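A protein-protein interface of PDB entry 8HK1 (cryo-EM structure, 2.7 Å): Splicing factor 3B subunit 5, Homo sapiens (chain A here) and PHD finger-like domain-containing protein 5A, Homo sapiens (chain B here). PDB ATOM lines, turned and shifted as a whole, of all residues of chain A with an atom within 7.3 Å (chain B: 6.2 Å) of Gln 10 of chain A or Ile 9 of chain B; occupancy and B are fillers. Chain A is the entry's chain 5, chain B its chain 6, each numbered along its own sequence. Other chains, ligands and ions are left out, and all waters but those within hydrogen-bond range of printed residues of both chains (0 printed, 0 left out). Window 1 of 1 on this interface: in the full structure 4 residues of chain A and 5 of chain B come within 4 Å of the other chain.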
ATOM      1  N   THR A   6      13.229  25.963 -13.550  1.00  0.00           N
ATOM      2  CA  THR A   6      14.328  25.966 -14.553  1.00  0.00           C
ATOM      3  C   THR A   6      14.892  24.551 -14.711  1.00  0.00           C
ATOM      4  O   THR A   6      15.797  24.379 -15.545  1.00  0.00           O
ATOM      5  CB  THR A   6      15.444  26.942 -14.160  1.00  0.00           C
ATOM      6  OG1 THR A   6      15.743  26.740 -12.778  1.00  0.00           O
ATOM      7  CG2 THR A   6      15.080  28.392 -14.398  1.00  0.00           C
ATOM      8  N   ILE A   7      14.343  23.579 -13.975  1.00  0.00           N
ATOM      9  CA  ILE A   7      14.830  22.166 -14.024  1.00  0.00           C
ATOM     10  C   ILE A   7      14.654  21.629 -15.449  1.00  0.00           C
ATOM     11  O   ILE A   7      15.581  20.960 -15.950  1.00  0.00           O
ATOM     12  CB  ILE A   7      14.064  21.296 -13.007  1.00  0.00           C
ATOM     13  CG1 ILE A   7      13.142  22.131 -12.116  1.00  0.00           C
ATOM     14  CG2 ILE A   7      15.016  20.427 -12.201  1.00  0.00           C
ATOM     15  CD1 ILE A   7      12.736  21.437 -10.836  1.00  0.00           C
ATOM     16  N   HIS A   8      13.517  21.944 -16.076  1.00  0.00           N
ATOM     17  CA  HIS A   8      13.216  21.485 -17.459  1.00  0.00           C
ATOM     18  C   HIS A   8      14.255  22.068 -18.420  1.00  0.00           C
ATOM     19  O   HIS A   8      14.731  21.325 -19.289  1.00  0.00           O
ATOM     20  CB  HIS A   8      11.790  21.903 -17.838  1.00  0.00           C
ATOM     21  CG  HIS A   8      10.976  22.336 -16.665  1.00  0.00           C
ATOM     22  ND1 HIS A   8      10.942  21.617 -15.486  1.00  0.00           N
ATOM     23  CD2 HIS A   8      10.175  23.407 -16.478  1.00  0.00           C
ATOM     24  CE1 HIS A   8      10.153  22.226 -14.624  1.00  0.00           C
ATOM     25  NE2 HIS A   8       9.668  23.326 -15.210  1.00  0.00           N
ATOM     26  N   SER A   9      14.593  23.348 -18.243  1.00  0.00           N
ATOM     27  CA  SER A   9      15.607  24.045 -19.077  1.00  0.00           C
ATOM     28  C   SER A   9      16.974  23.380 -18.882  1.00  0.00           C
ATOM     29  O   SER A   9      17.695  23.218 -19.883  1.00  0.00           O
ATOM     30  CB  SER A   9      15.663  25.510 -18.739  1.00  0.00           C
ATOM     31  OG  SER A   9      16.463  25.731 -17.588  1.00  0.00           O
ATOM     32  N   GLN A  10      17.313  23.011 -17.641  1.00  0.00           N
ATOM     33  CA  GLN A  10      18.607  22.326 -17.372  1.00  0.00           C
ATOM     34  C   GLN A  10      18.612  20.982 -18.100  1.00  0.00           C
ATOM     35  O   GLN A  10      19.647  20.633 -18.695  1.00  0.00           O
ATOM     36  CB  GLN A  10      18.773  22.014 -15.888  1.00  0.00           C
ATOM     37  CG  GLN A  10      20.114  21.374 -15.564  1.00  0.00           C
ATOM     38  CD  GLN A  10      20.056  20.515 -14.327  1.00  0.00           C
ATOM     39  OE1 GLN A  10      18.985  20.188 -13.823  1.00  0.00           O
ATOM     40  NE2 GLN A  10      21.222  20.170 -13.806  1.00  0.00           N
ATOM     41  N   LEU A  11      17.477  20.276 -18.068  1.00  0.00           N
ATOM     42  CA  LEU A  11      17.357  18.966 -18.760  1.00  0.00           C
ATOM     43  C   LEU A  11      17.568  19.200 -20.260  1.00  0.00           C
ATOM     44  O   LEU A  11      18.314  18.420 -20.880  1.00  0.00           O
ATOM     45  CB  LEU A  11      15.961  18.405 -18.474  1.00  0.00           C
ATOM     46  CG  LEU A  11      15.727  16.957 -18.897  1.00  0.00           C
ATOM     47  CD1 LEU A  11      15.725  16.826 -20.411  1.00  0.00           C
ATOM     48  CD2 LEU A  11      16.763  16.033 -18.278  1.00  0.00           C
ATOM     49  N   GLU A  12      16.972  20.269 -20.799  1.00  0.00           N
ATOM     50  CA  GLU A  12      17.125  20.633 -22.230  1.00  0.00           C
ATOM     51  C   GLU A  12      18.589  20.989 -22.513  1.00  0.00           C
ATOM     52  O   GLU A  12      18.993  20.882 -23.688  1.00  0.00           O
ATOM     53  CB  GLU A  12      16.212  21.804 -22.600  1.00  0.00           C
ATOM     54  CG  GLU A  12      14.733  21.480 -22.502  1.00  0.00           C
ATOM     55  CD  GLU A  12      13.812  22.679 -22.642  1.00  0.00           C
ATOM     56  OE1 GLU A  12      13.903  23.379 -23.669  1.00  0.00           O
ATOM     57  OE2 GLU A  12      13.009  22.916 -21.719  1.00  0.00           O
ATOM     58  N   HIS A  13      19.346  21.435 -21.501  1.00  0.00           N
ATOM     59  CA  HIS A  13      20.772  21.764 -21.773  1.00  0.00           C
ATOM     60  C   HIS A  13      21.656  20.515 -21.637  1.00  0.00           C
ATOM     61  O   HIS A  13      22.667  20.434 -22.357  1.00  0.00           O
ATOM     62  CB  HIS A  13      21.223  22.892 -20.832  1.00  0.00           C
ATOM     63  CG  HIS A  13      22.549  23.481 -21.175  1.00  0.00           C
ATOM     64  ND1 HIS A  13      23.728  23.003 -20.639  1.00  0.00           N
ATOM     65  CD2 HIS A  13      22.888  24.508 -21.984  1.00  0.00           C
ATOM     66  CE1 HIS A  13      24.738  23.705 -21.108  1.00  0.00           C
ATOM     67  NE2 HIS A  13      24.250  24.636 -21.935  1.00  0.00           N
ATOM     68  N   LEU A  14      21.283  19.588 -20.747  1.00  0.00           N
ATOM     69  CA  LEU A  14      22.041  18.339 -20.476  1.00  0.00           C
ATOM     70  C   LEU A  14      21.809  17.351 -21.623  1.00  0.00           C
ATOM     71  O   LEU A  14      22.762  16.647 -21.997  1.00  0.00           O
ATOM     72  CB  LEU A  14      21.590  17.765 -19.131  1.00  0.00           C
ATOM     73  CG  LEU A  14      22.068  18.539 -17.903  1.00  0.00           C
ATOM     74  CD1 LEU A  14      21.521  17.925 -16.624  1.00  0.00           C
ATOM     75  CD2 LEU A  14      23.585  18.605 -17.854  1.00  0.00           C
ATOM     76  N   GLN A  15      20.575  17.293 -22.133  1.00  0.00           N
ATOM     77  CA  GLN A  15      20.234  16.400 -23.271  1.00  0.00           C
ATOM     78  C   GLN A  15      21.042  16.855 -24.487  1.00  0.00           C
ATOM     79  O   GLN A  15      21.584  15.986 -25.189  1.00  0.00           O
ATOM     80  CB  GLN A  15      18.730  16.438 -23.540  1.00  0.00           C
ATOM     81  CG  GLN A  15      17.918  15.667 -22.510  1.00  0.00           C
ATOM     82  CD  GLN A  15      16.578  15.235 -23.051  1.00  0.00           C
ATOM     83  OE1 GLN A  15      16.074  15.787 -24.026  1.00  0.00           O
ATOM     84  NE2 GLN A  15      15.988  14.237 -22.416  1.00  0.00           N
ATOM     85  N   SER A  16      21.145  18.172 -24.693  1.00  0.00           N
ATOM     86  CA  SER A  16      21.946  18.722 -25.817  1.00  0.00           C
ATOM     87  C   SER A  16      23.416  18.336 -25.616  1.00  0.00           C
ATOM     88  O   SER A  16      24.073  17.951 -26.600  1.00  0.00           O
ATOM     89  CB  SER A  16      21.787  20.214 -25.900  1.00  0.00           C
ATOM     90  OG  SER A  16      22.699  20.765 -26.838  1.00  0.00           O
ATOM     91  N   ASP B   7      14.760  28.000  -9.740  1.00  0.00           N
ATOM     92  CA  ASP B   7      16.185  27.819  -9.502  1.00  0.00           C
ATOM     93  C   ASP B   7      16.452  26.501  -8.784  1.00  0.00           C
ATOM     94  O   ASP B   7      17.547  26.267  -8.272  1.00  0.00           O
ATOM     95  CB  ASP B   7      16.748  28.995  -8.701  1.00  0.00           C
ATOM     96  CG  ASP B   7      16.576  30.321  -9.419  1.00  0.00           C
ATOM     97  OD1 ASP B   7      15.434  30.830  -9.461  1.00  0.00           O
ATOM     98  OD2 ASP B   7      17.576  30.858  -9.937  1.00  0.00           O
ATOM     99  N   LEU B   8      15.435  25.642  -8.747  1.00  0.00           N
ATOM    100  CA  LEU B   8      15.612  24.274  -8.277  1.00  0.00           C
ATOM    101  C   LEU B   8      16.301  23.453  -9.360  1.00  0.00           C
ATOM    102  O   LEU B   8      15.646  22.920 -10.264  1.00  0.00           O
ATOM    103  CB  LEU B   8      14.264  23.665  -7.899  1.00  0.00           C
ATOM    104  CG  LEU B   8      13.591  24.242  -6.649  1.00  0.00           C
ATOM    105  CD1 LEU B   8      12.748  23.198  -5.949  1.00  0.00           C
ATOM    106  CD2 LEU B   8      14.625  24.814  -5.680  1.00  0.00           C
ATOM    107  N   ILE B   9      17.627  23.355  -9.270  1.00  0.00           N
ATOM    108  CA  ILE B   9      18.436  22.676 -10.274  1.00  0.00           C
ATOM    109  C   ILE B   9      19.340  21.683  -9.560  1.00  0.00           C
ATOM    110  O   ILE B   9      19.871  21.964  -8.482  1.00  0.00           O
ATOM    111  CB  ILE B   9      19.256  23.691 -11.107  1.00  0.00           C
ATOM    112  CG1 ILE B   9      18.322  24.594 -11.920  1.00  0.00           C
ATOM    113  CG2 ILE B   9      20.249  22.979 -12.010  1.00  0.00           C
ATOM    114  CD1 ILE B   9      18.118  24.157 -13.352  1.00  0.00           C
ATOM    115  N   PHE B  10      19.507  20.509 -10.163  1.00  0.00           N
ATOM    116  CA  PHE B  10      20.424  19.515  -9.633  1.00  0.00           C
ATOM    117  C   PHE B  10      21.868  19.911  -9.928  1.00  0.00           C
ATOM    118  O   PHE B  10      22.151  20.648 -10.875  1.00  0.00           O
ATOM    119  CB  PHE B  10      20.120  18.143 -10.232  1.00  0.00           C
ATOM    120  CG  PHE B  10      18.777  17.595  -9.841  1.00  0.00           C
ATOM    121  CD1 PHE B  10      18.519  17.227  -8.535  1.00  0.00           C
ATOM    122  CD2 PHE B  10      17.771  17.461 -10.780  1.00  0.00           C
ATOM    123  CE1 PHE B  10      17.288  16.720  -8.178  1.00  0.00           C
ATOM    124  CE2 PHE B  10      16.540  16.959 -10.423  1.00  0.00           C
ATOM    125  CZ  PHE B  10      16.299  16.590  -9.119  1.00  0.00           C
ATOM    126  N   CYS B  11      22.789  19.415  -9.102  1.00  0.00           N
ATOM    127  CA  CYS B  11      24.201  19.748  -9.282  1.00  0.00           C
ATOM    128  C   CYS B  11      24.773  19.092 -10.537  1.00  0.00           C
ATOM    129  O   CYS B  11      25.344  19.773 -11.395  1.00  0.00           O
ATOM    130  CB  CYS B  11      24.997  19.342  -8.042  1.00  0.00           C
ATOM    131  SG  CYS B  11      26.778  19.576  -8.195  1.00  0.00           S
ATOM    132  N   ARG B  12      24.642  17.768 -10.647  1.00  0.00           N
ATOM    133  CA  ARG B  12      24.975  17.010 -11.855  1.00  0.00           C
ATOM    134  C   ARG B  12      26.481  17.013 -12.134  1.00  0.00           C
ATOM    135  O   ARG B  12      26.929  17.013 -13.280  1.00  0.00           O
ATOM    136  CB  ARG B  12      24.190  17.532 -13.063  1.00  0.00           C
ATOM    137  CG  ARG B  12      22.693  17.310 -12.980  1.00  0.00           C
ATOM    138  CD  ARG B  12      22.365  15.920 -12.471  1.00  0.00           C
ATOM    139  NE  ARG B  12      20.974  15.564 -12.728  1.00  0.00           N
ATOM    140  CZ  ARG B  12      20.318  14.603 -12.088  1.00  0.00           C
ATOM    141  NH1 ARG B  12      20.928  13.896 -11.146  1.00  0.00           N
ATOM    142  NH2 ARG B  12      19.052  14.349 -12.387  1.00  0.00           N
ATOM    143  N   LYS B  87      22.283  16.742  -5.634  1.00  0.00           N
ATOM    144  CA  LYS B  87      22.033  17.768  -4.627  1.00  0.00           C
ATOM    145  C   LYS B  87      21.279  18.940  -5.245  1.00  0.00           C
ATOM    146  O   LYS B  87      21.664  19.445  -6.303  1.00  0.00           O
ATOM    147  CB  LYS B  87      23.349  18.240  -4.023  1.00  0.00           C
ATOM    148  CG  LYS B  87      23.265  18.560  -2.553  1.00  0.00           C
ATOM    149  CD  LYS B  87      23.275  20.058  -2.332  1.00  0.00           C
ATOM    150  CE  LYS B  87      23.738  20.409  -0.930  1.00  0.00           C
ATOM    151  NZ  LYS B  87      23.422  21.825  -0.609  1.00  0.00           N
ATOM    152  N   ILE B  88      20.203  19.372  -4.583  1.00  0.00           N
ATOM    153  CA  ILE B  88      19.483  20.555  -5.035  1.00  0.00           C
ATOM    154  C   ILE B  88      20.294  21.794  -4.696  1.00  0.00           C
ATOM    155  O   ILE B  88      20.569  22.067  -3.522  1.00  0.00           O
ATOM    156  CB  ILE B  88      18.084  20.616  -4.397  1.00  0.00           C
ATOM    157  CG1 ILE B  88      17.295  19.343  -4.698  1.00  0.00           C
ATOM    158  CG2 ILE B  88      17.336  21.849  -4.877  1.00  0.00           C
ATOM    159  CD1 ILE B  88      16.598  19.357  -6.026  1.00  0.00           C
ATOM    160  N   VAL B  89      20.672  22.552  -5.721  1.00  0.00           N
ATOM    161  CA  VAL B  89      21.468  23.760  -5.559  1.00  0.00           C
ATOM    162  C   VAL B  89      20.673  24.944  -6.095  1.00  0.00           C
ATOM    163  O   VAL B  89      20.018  24.845  -7.139  1.00  0.00           O
ATOM    164  CB  VAL B  89      22.844  23.636  -6.254  1.00  0.00           C
ATOM    165  CG1 VAL B  89      23.604  22.434  -5.713  1.00  0.00           C
ATOM    166  CG2 VAL B  89      22.694  23.512  -7.763  1.00  0.00           C
ATOM    167  N   ASN B  90      20.694  26.050  -5.356  1.00  0.00           N
ATOM    168  CA  ASN B  90      20.008  27.257  -5.787  1.00  0.00           C
ATOM    169  C   ASN B  90      21.008  28.346  -6.163  1.00  0.00           C
ATOM    170  O   ASN B  90      22.066  28.497  -5.549  1.00  0.00           O
ATOM    171  CB  ASN B  90      19.070  27.774  -4.695  1.00  0.00           C
ATOM    172  CG  ASN B  90      17.812  26.943  -4.572  1.00  0.00           C
ATOM    173  OD1 ASN B  90      16.896  27.051  -5.401  1.00  0.00           O
ATOM    174  ND2 ASN B  90      17.746  26.116  -3.524  1.00  0.00           N
ATOM    175  N   LEU B  91      20.651  29.111  -7.189  1.00  0.00           N
ATOM    176  CA  LEU B  91      21.517  30.155  -7.718  1.00  0.00           C
ATOM    177  C   LEU B  91      20.930  31.539  -7.455  1.00  0.00           C
ATOM    178  O   LEU B  91      21.206  32.162  -6.432  1.00  0.00           O
ATOM    179  CB  LEU B  91      21.730  29.948  -9.217  1.00  0.00           C
ATOM    180  CG  LEU B  91      22.469  28.662  -9.596  1.00  0.00           C
ATOM    181  CD1 LEU B  91      21.745  27.935 -10.720  1.00  0.00           C
ATOM    182  CD2 LEU B  91      23.903  28.972  -9.992  1.00  0.00           C
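The side-chain amide oxygen (OD1) of Asn 90 of chain B lies close to the backbone carbonyl oxygen (O) of Asp 7 of chain B (3.0 Å).
The backbone NH (N) of Val 89 of chain B lies within hydrogen-bond range of the backbone carbonyl oxygen (O) of Ile 9 of chain B (2.9 Å).
The side-chain hydroxyl (OG) of Ser 9 of chain A sits at hydrogen-bond distance from the backbone carbonyl oxygen (O) of Thr 6 of chain A, 2.5 Å away.
The backbone carbonyl oxygen (O) of Phe 10 of chain B sits at hydrogen-bond distance from the side-chain amide nitrogen (NE2) of Gln 10 of chain A, 3.1 Å away.
The side-chain hydroxyl (OG1) of Thr 6 of chain A lies within hydrogen-bond range of the backbone NH (N) of Asp 7 of chain B, 3.4 Å away.
Printed residues of chain B within 4 Å of Gln 10 of chain A: Ile 9 (3.4 Å), Phe 10 (3.1 Å) and Arg 12 (3.3 Å).
Of the printed residues of chain B, Leu 14 of chain A touches Arg 12 (3.9 Å).
Ile 9 of chain B touches three residues of chain A.
Of the printed residues of chain A, Arg 12 of chain B touches Gln 10 (3.3 Å) and Leu 14 (3.9 Å).
The nearest residue of chain B that does not touch Gln 10 of chain A is Cys 11 of chain B (4.8 Å).
Of the 11 printed residues of chain A, 4 touch a printed residue of chain B.
Hydrophobic or aromatic side chains of chain B within 4 Å of the printed part of chain A: Leu 8 and Ile 9.
Among the printed residues, merely in contact across the chains: Thr 6 of chain A with Ile 9 of chain B (3.2 Å), Ile 7 of chain A with Leu 8 of chain B (3.2 Å), Ile 7 of chain A with Ile 9 of chain B (3.9 Å), Gln 10 of chain A with Ile 9 of chain B (3.4 Å), Gln 10 of chain A with Arg 12 of chain B (3.3 Å) and Leu 14 of chain A with Arg 12 of chain B (3.9 Å).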
